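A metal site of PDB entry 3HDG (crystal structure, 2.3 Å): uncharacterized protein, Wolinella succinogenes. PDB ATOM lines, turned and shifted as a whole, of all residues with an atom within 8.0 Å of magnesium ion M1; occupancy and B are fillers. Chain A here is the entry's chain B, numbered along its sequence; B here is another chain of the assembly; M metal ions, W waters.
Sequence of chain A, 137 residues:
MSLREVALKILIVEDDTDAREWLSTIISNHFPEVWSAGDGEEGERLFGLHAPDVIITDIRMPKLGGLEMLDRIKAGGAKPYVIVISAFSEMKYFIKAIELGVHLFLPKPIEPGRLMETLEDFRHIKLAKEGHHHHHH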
ATOM      1  N   VAL A  13      10.031  11.503   2.867  1.00  0.00           N
ATOM      2  CA  VAL A  13      10.639  11.282   1.559  1.00  0.00           C
ATOM      3  C   VAL A  13       9.738  11.955   0.502  1.00  0.00           C
ATOM      4  O   VAL A  13       8.695  11.422   0.133  1.00  0.00           O
ATOM      5  CB  VAL A  13      10.779   9.778   1.235  1.00  0.00           C
ATOM      6  CG1 VAL A  13      11.655   9.587  -0.016  1.00  0.00           C
ATOM      7  CG2 VAL A  13      11.403   9.056   2.433  1.00  0.00           C
ATOM      8  N   GLU A  14      10.162  13.142   0.059  1.00  0.00           N
ATOM      9  CA  GLU A  14       9.428  13.925  -0.941  1.00  0.00           C
ATOM     10  C   GLU A  14      10.444  14.537  -1.928  1.00  0.00           C
ATOM     11  O   GLU A  14      11.410  15.179  -1.520  1.00  0.00           O
ATOM     12  CB  GLU A  14       8.613  15.028  -0.236  1.00  0.00           C
ATOM     13  CG  GLU A  14       8.134  16.168  -1.123  1.00  0.00           C
ATOM     14  CD  GLU A  14       7.168  15.735  -2.230  1.00  0.00           C
ATOM     15  OE1 GLU A  14       6.038  15.316  -1.909  1.00  0.00           O
ATOM     16  OE2 GLU A  14       7.554  15.814  -3.415  1.00  0.00           O
ATOM     17  N   ASP A  15      10.217  14.344  -3.229  1.00  0.00           N
ATOM     18  CA  ASP A  15      11.148  14.876  -4.214  1.00  0.00           C
ATOM     19  C   ASP A  15      11.034  16.375  -4.484  1.00  0.00           C
ATOM     20  O   ASP A  15      11.958  16.978  -5.013  1.00  0.00           O
ATOM     21  CB  ASP A  15      11.066  14.099  -5.524  1.00  0.00           C
ATOM     22  CG  ASP A  15       9.716  14.223  -6.203  1.00  0.00           C
ATOM     23  OD1 ASP A  15       8.835  14.949  -5.686  1.00  0.00           O
ATOM     24  OD2 ASP A  15       9.549  13.584  -7.268  1.00  0.00           O
ATOM     25  N   ASP A  16       9.926  16.984  -4.118  1.00  0.00           N
ATOM     26  CA  ASP A  16       9.791  18.400  -4.342  1.00  0.00           C
ATOM     27  C   ASP A  16      10.460  19.157  -3.192  1.00  0.00           C
ATOM     28  O   ASP A  16      10.109  18.968  -2.025  1.00  0.00           O
ATOM     29  CB  ASP A  16       8.330  18.786  -4.474  1.00  0.00           C
ATOM     30  CG  ASP A  16       8.151  20.227  -4.918  1.00  0.00           C
ATOM     31  OD1 ASP A  16       8.670  20.559  -6.012  1.00  0.00           O
ATOM     32  OD2 ASP A  16       7.527  21.004  -4.181  1.00  0.00           O
ATOM     33  N   THR A  17      11.423  20.002  -3.526  1.00  0.00           N
ATOM     34  CA  THR A  17      12.134  20.778  -2.515  1.00  0.00           C
ATOM     35  C   THR A  17      11.217  21.595  -1.620  1.00  0.00           C
ATOM     36  O   THR A  17      11.342  21.562  -0.394  1.00  0.00           O
ATOM     37  CB  THR A  17      13.153  21.713  -3.177  1.00  0.00           C
ATOM     38  OG1 THR A  17      14.237  20.931  -3.699  1.00  0.00           O
ATOM     39  CG2 THR A  17      13.681  22.739  -2.173  1.00  0.00           C
ATOM     40  N   ALA A  19       7.847  21.322  -1.075  1.00  0.00           N
ATOM     41  CA  ALA A  19       6.976  20.491  -0.271  1.00  0.00           C
ATOM     42  C   ALA A  19       7.717  19.721   0.828  1.00  0.00           C
ATOM     43  O   ALA A  19       7.177  19.527   1.913  1.00  0.00           O
ATOM     44  CB  ALA A  19       6.202  19.515  -1.164  1.00  0.00           C
ATOM     45  N   ARG A  20       8.942  19.306   0.537  1.00  0.00           N
ATOM     46  CA  ARG A  20       9.741  18.568   1.504  1.00  0.00           C
ATOM     47  C   ARG A  20      10.089  19.431   2.717  1.00  0.00           C
ATOM     48  O   ARG A  20       9.914  19.020   3.856  1.00  0.00           O
ATOM     49  CB  ARG A  20      11.027  18.048   0.849  1.00  0.00           C
ATOM     50  CG  ARG A  20      11.822  17.099   1.736  1.00  0.00           C
ATOM     51  CD  ARG A  20      13.018  16.462   0.996  1.00  0.00           C
ATOM     52  NE  ARG A  20      13.991  17.459   0.520  1.00  0.00           N
ATOM     53  CZ  ARG A  20      14.101  17.856  -0.742  1.00  0.00           C
ATOM     54  NH1 ARG A  20      13.300  17.356  -1.685  1.00  0.00           N
ATOM     55  NH2 ARG A  20      15.037  18.740  -1.088  1.00  0.00           N
ATOM     56  N   GLY A  38      15.084  13.309  -0.524  1.00  0.00           N
ATOM     57  CA  GLY A  38      14.478  13.715  -1.792  1.00  0.00           C
ATOM     58  C   GLY A  38      14.218  12.646  -2.849  1.00  0.00           C
ATOM     59  O   GLY A  38      13.739  12.971  -3.927  1.00  0.00           O
ATOM     60  N   THR A  57       6.070   9.128   2.615  1.00  0.00           N
ATOM     61  CA  THR A  57       6.716   9.091   1.316  1.00  0.00           C
ATOM     62  C   THR A  57       5.892   9.264   0.040  1.00  0.00           C
ATOM     63  O   THR A  57       4.709   8.884  -0.042  1.00  0.00           O
ATOM     64  CB  THR A  57       7.532   7.797   1.149  1.00  0.00           C
ATOM     65  OG1 THR A  57       8.179   7.793  -0.120  1.00  0.00           O
ATOM     66  CG2 THR A  57       6.622   6.568   1.261  1.00  0.00           C
ATOM     67  N   ASP A  58       6.549   9.857  -0.947  1.00  0.00           N
ATOM     68  CA  ASP A  58       5.988  10.081  -2.265  1.00  0.00           C
ATOM     69  C   ASP A  58       6.017   8.715  -2.947  1.00  0.00           C
ATOM     70  O   ASP A  58       6.657   7.782  -2.458  1.00  0.00           O
ATOM     71  CB  ASP A  58       6.906  11.010  -3.056  1.00  0.00           C
ATOM     72  CG  ASP A  58       6.187  12.209  -3.620  1.00  0.00           C
ATOM     73  OD1 ASP A  58       4.942  12.226  -3.609  1.00  0.00           O
ATOM     74  OD2 ASP A  58       6.871  13.137  -4.097  1.00  0.00           O
ATOM     75  N   ILE A  59       5.330   8.609  -4.077  1.00  0.00           N
ATOM     76  CA  ILE A  59       5.353   7.376  -4.824  1.00  0.00           C
ATOM     77  C   ILE A  59       6.289   7.585  -6.014  1.00  0.00           C
ATOM     78  O   ILE A  59       7.308   6.931  -6.114  1.00  0.00           O
ATOM     79  CB  ILE A  59       3.956   6.965  -5.294  1.00  0.00           C
ATOM     80  CG1 ILE A  59       3.101   6.596  -4.073  1.00  0.00           C
ATOM     81  CG2 ILE A  59       4.056   5.770  -6.243  1.00  0.00           C
ATOM     82  CD1 ILE A  59       1.679   6.181  -4.424  1.00  0.00           C
ATOM     83  N   ARG A  60       5.945   8.501  -6.908  1.00  0.00           N
ATOM     84  CA  ARG A  60       6.806   8.748  -8.056  1.00  0.00           C
ATOM     85  C   ARG A  60       7.931   9.706  -7.687  1.00  0.00           C
ATOM     86  O   ARG A  60       7.695  10.849  -7.317  1.00  0.00           O
ATOM     87  CB  ARG A  60       6.005   9.283  -9.259  1.00  0.00           C
ATOM     88  CG  ARG A  60       5.125   8.216  -9.924  1.00  0.00           C
ATOM     89  CD  ARG A  60       4.656   8.678 -11.293  1.00  0.00           C
ATOM     90  NE  ARG A  60       5.748   8.730 -12.261  1.00  0.00           N
ATOM     91  CZ  ARG A  60       6.214   7.682 -12.934  1.00  0.00           C
ATOM     92  NH1 ARG A  60       5.677   6.482 -12.756  1.00  0.00           N
ATOM     93  NH2 ARG A  60       7.224   7.831 -13.793  1.00  0.00           N
ATOM     94  N   MET A  61       9.160   9.210  -7.784  1.00  0.00           N
ATOM     95  CA  MET A  61      10.360   9.968  -7.444  1.00  0.00           C
ATOM     96  C   MET A  61      11.548   9.477  -8.256  1.00  0.00           C
ATOM     97  O   MET A  61      11.582   8.335  -8.695  1.00  0.00           O
ATOM     98  CB  MET A  61      10.757   9.782  -5.979  1.00  0.00           C
ATOM     99  CG  MET A  61       9.766  10.231  -4.946  1.00  0.00           C
ATOM    100  SD  MET A  61      10.577  10.061  -3.174  1.00  0.00           S
ATOM    101  CE  MET A  61      10.660   8.129  -3.051  1.00  0.00           C
ATOM    102  N   PRO A  62      12.556  10.345  -8.418  1.00  0.00           N
ATOM    103  CA  PRO A  62      13.755  10.005  -9.174  1.00  0.00           C
ATOM    104  C   PRO A  62      14.570   8.917  -8.476  1.00  0.00           C
ATOM    105  O   PRO A  62      14.398   8.673  -7.280  1.00  0.00           O
ATOM    106  CB  PRO A  62      14.502  11.347  -9.257  1.00  0.00           C
ATOM    107  CG  PRO A  62      14.083  12.038  -7.989  1.00  0.00           C
ATOM    108  CD  PRO A  62      12.616  11.727  -7.904  1.00  0.00           C
ATOM    109  N   ILE A  85       1.980   9.824   0.299  1.00  0.00           N
ATOM    110  CA  ILE A  85       1.627  11.085  -0.318  1.00  0.00           C
ATOM    111  C   ILE A  85       1.138  10.712  -1.717  1.00  0.00           C
ATOM    112  O   ILE A  85       1.936  10.408  -2.607  1.00  0.00           O
ATOM    113  CB  ILE A  85       2.868  12.007  -0.480  1.00  0.00           C
ATOM    114  CG1 ILE A  85       3.479  12.338   0.877  1.00  0.00           C
ATOM    115  CG2 ILE A  85       2.467  13.299  -1.168  1.00  0.00           C
ATOM    116  CD1 ILE A  85       4.705  13.276   0.779  1.00  0.00           C
ATOM    117  N   LYS A 108      -2.815  15.025  -1.799  1.00  0.00           N
ATOM    118  CA  LYS A 108      -2.172  16.325  -1.942  1.00  0.00           C
ATOM    119  C   LYS A 108      -3.270  17.252  -2.482  1.00  0.00           C
ATOM    120  O   LYS A 108      -4.143  16.793  -3.213  1.00  0.00           O
ATOM    121  CB  LYS A 108      -1.019  16.253  -2.942  1.00  0.00           C
ATOM    122  CG  LYS A 108       0.020  15.166  -2.650  1.00  0.00           C
ATOM    123  CD  LYS A 108       1.410  15.546  -3.215  1.00  0.00           C
ATOM    124  CE  LYS A 108       1.421  15.680  -4.745  1.00  0.00           C
ATOM    125  NZ  LYS A 108       2.713  16.261  -5.261  1.00  0.00           N
ATOM    126  N   GLU B  14      10.477  21.336 -13.305  1.00  0.00           N
ATOM    127  CA  GLU B  14       9.871  21.166 -11.993  1.00  0.00           C
ATOM    128  C   GLU B  14      10.480  19.942 -11.305  1.00  0.00           C
ATOM    129  O   GLU B  14      10.541  18.864 -11.903  1.00  0.00           O
ATOM    130  CB  GLU B  14       8.350  20.979 -12.152  1.00  0.00           C
ATOM    131  CG  GLU B  14       7.620  20.471 -10.914  1.00  0.00           C
ATOM    132  CD  GLU B  14       7.697  21.430  -9.745  1.00  0.00           C
ATOM    133  OE1 GLU B  14       7.303  22.598  -9.907  1.00  0.00           O
ATOM    134  OE2 GLU B  14       8.169  21.017  -8.664  1.00  0.00           O
ATOM    135  N   ASP B  15      10.910  20.094 -10.059  1.00  0.00           N
ATOM    136  CA  ASP B  15      11.528  18.988  -9.330  1.00  0.00           C
ATOM    137  C   ASP B  15      10.544  17.958  -8.778  1.00  0.00           C
ATOM    138  O   ASP B  15      10.929  16.844  -8.451  1.00  0.00           O
ATOM    139  CB  ASP B  15      12.468  19.505  -8.227  1.00  0.00           C
ATOM    140  CG  ASP B  15      11.793  20.481  -7.271  1.00  0.00           C
ATOM    141  OD1 ASP B  15      10.884  21.205  -7.696  1.00  0.00           O
ATOM    142  OD2 ASP B  15      12.216  20.548  -6.091  1.00  0.00           O
ATOM    143  N   ASP B  16       9.271  18.329  -8.667  1.00  0.00           N
ATOM    144  CA  ASP B  16       8.289  17.361  -8.197  1.00  0.00           C
ATOM    145  C   ASP B  16       7.875  16.512  -9.417  1.00  0.00           C
ATOM    146  O   ASP B  16       7.383  17.046 -10.416  1.00  0.00           O
ATOM    147  CB  ASP B  16       7.056  18.050  -7.625  1.00  0.00           C
ATOM    148  CG  ASP B  16       6.095  17.073  -6.993  1.00  0.00           C
ATOM    149  OD1 ASP B  16       6.415  16.549  -5.898  1.00  0.00           O
ATOM    150  OD2 ASP B  16       5.028  16.805  -7.584  1.00  0.00           O
ATOM    151  N   THR B  17       8.077  15.202  -9.322  1.00  0.00           N
ATOM    152  CA  THR B  17       7.759  14.305 -10.436  1.00  0.00           C
ATOM    153  C   THR B  17       6.289  14.285 -10.805  1.00  0.00           C
ATOM    154  O   THR B  17       5.942  14.382 -11.990  1.00  0.00           O
ATOM    155  CB  THR B  17       8.222  12.851 -10.129  1.00  0.00           C
ATOM    156  OG1 THR B  17       9.665  12.812 -10.067  1.00  0.00           O
ATOM    157  CG2 THR B  17       7.742  11.882 -11.214  1.00  0.00           C
ATOM    158  N   ASP B  18       5.427  14.195  -9.800  1.00  0.00           N
ATOM    159  CA  ASP B  18       3.984  14.163 -10.042  1.00  0.00           C
ATOM    160  C   ASP B  18       3.498  15.391 -10.791  1.00  0.00           C
ATOM    161  O   ASP B  18       2.809  15.280 -11.793  1.00  0.00           O
ATOM    162  CB  ASP B  18       3.217  14.025  -8.718  1.00  0.00           C
ATOM    163  CG  ASP B  18       3.558  12.741  -7.974  1.00  0.00           C
ATOM    164  OD1 ASP B  18       3.560  11.675  -8.615  1.00  0.00           O
ATOM    165  OD2 ASP B  18       3.800  12.803  -6.742  1.00  0.00           O
ATOM    166  N   ALA B  19       3.859  16.573 -10.300  1.00  0.00           N
ATOM    167  CA  ALA B  19       3.421  17.813 -10.928  1.00  0.00           C
ATOM    168  C   ALA B  19       4.047  17.975 -12.303  1.00  0.00           C
ATOM    169  O   ALA B  19       3.411  18.482 -13.221  1.00  0.00           O
ATOM    170  CB  ALA B  19       3.788  19.017 -10.047  1.00  0.00           C
ATOM    171  N   ARG B  20       5.295  17.528 -12.447  1.00  0.00           N
ATOM    172  CA  ARG B  20       5.987  17.647 -13.702  1.00  0.00           C
ATOM    173  C   ARG B  20       5.310  16.788 -14.772  1.00  0.00           C
ATOM    174  O   ARG B  20       5.060  17.250 -15.875  1.00  0.00           O
ATOM    175  CB  ARG B  20       7.467  17.251 -13.563  1.00  0.00           C
ATOM    176  CG  ARG B  20       8.251  17.435 -14.849  1.00  0.00           C
ATOM    177  CD  ARG B  20       9.721  17.022 -14.725  1.00  0.00           C
ATOM    178  NE  ARG B  20       9.877  15.599 -14.394  1.00  0.00           N
ATOM    179  CZ  ARG B  20      10.252  15.142 -13.196  1.00  0.00           C
ATOM    180  NH1 ARG B  20      10.519  15.993 -12.205  1.00  0.00           N
ATOM    181  NH2 ARG B  20      10.364  13.831 -12.996  1.00  0.00           N
ATOM    182  N   LYS B 108       1.216  27.300  -7.295  1.00  0.00           N
ATOM    183  CA  LYS B 108       0.497  26.078  -6.959  1.00  0.00           C
ATOM    184  C   LYS B 108      -0.539  26.286  -5.873  1.00  0.00           C
ATOM    185  O   LYS B 108      -0.380  27.147  -4.997  1.00  0.00           O
ATOM    186  CB  LYS B 108       1.488  25.020  -6.511  1.00  0.00           C
ATOM    187  CG  LYS B 108       2.537  24.688  -7.546  1.00  0.00           C
ATOM    188  CD  LYS B 108       3.499  23.664  -6.998  1.00  0.00           C
ATOM    189  CE  LYS B 108       4.455  23.166  -8.070  1.00  0.00           C
ATOM    190  NZ  LYS B 108       5.312  22.098  -7.512  1.00  0.00           N
HETATM  191 MG    MG M   1       6.859  14.841  -5.170  1.00  0.00          MG
HETATM  192 MG    MG M   2       9.324  22.105  -7.001  1.00  0.00          MG
HETATM  193  O   HOH W   1       4.866  14.580  -4.194  1.00  0.00           O
HETATM  194  O   HOH W   2       6.396  13.251  -6.799  1.00  0.00           O
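Residues that only touch magnesium ion M1: Asp 16 of chain A (3.9 Å) and Asp 18 of chain B (3.998 Å).
OD2 of Asp 16 of chain B lies close to N of Asp 18 of chain B (3.4 Å).
The side-chain carboxylate (OD2) of Asp 16 of chain B is in salt-bridge range of the side-chain amino group (NZ) of Lys 108 of chain A.
The side-chain carboxylate of Asp 16 of chain B sits at hydrogen-bond distance from the backbone NH of Ala 19 of chain B.
N of Asp 16 of chain B lies close to OE2 of Glu 14 of chain B, 2.9 Å away.
The side-chain carboxylate (OD2) of Asp 15 of chain A is in hydrogen-bond range of the side-chain hydroxyl (OG1) of Thr 17 of chain B (2.9 Å).
OE2 of Glu 14 of chain A sits close to N of Asp 16 of chain A.
The side-chain carboxylate (OD2) of Asp 16 of chain A sits at hydrogen-bond distance from the backbone NH (N) of Ala 19 of chain A, 3.1 Å away.
The side-chain carboxylate (OD2) of Asp 18 of chain B lies within salt-bridge range of the side-chain amino group (NZ) of Lys 108 of chain A, at 3.9 Å.
Magnesium ion M1 is bound by OD1 of Asp 16 of chain B (1.9 Å), OD2 of Asp 58 (2.0 Å), OD1 of Asp 15 of chain A (2.0 Å), OE2 of Glu 14 of chain A (2.1 Å), water W1 (2.2 Å) and water W2 (2.3 Å).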
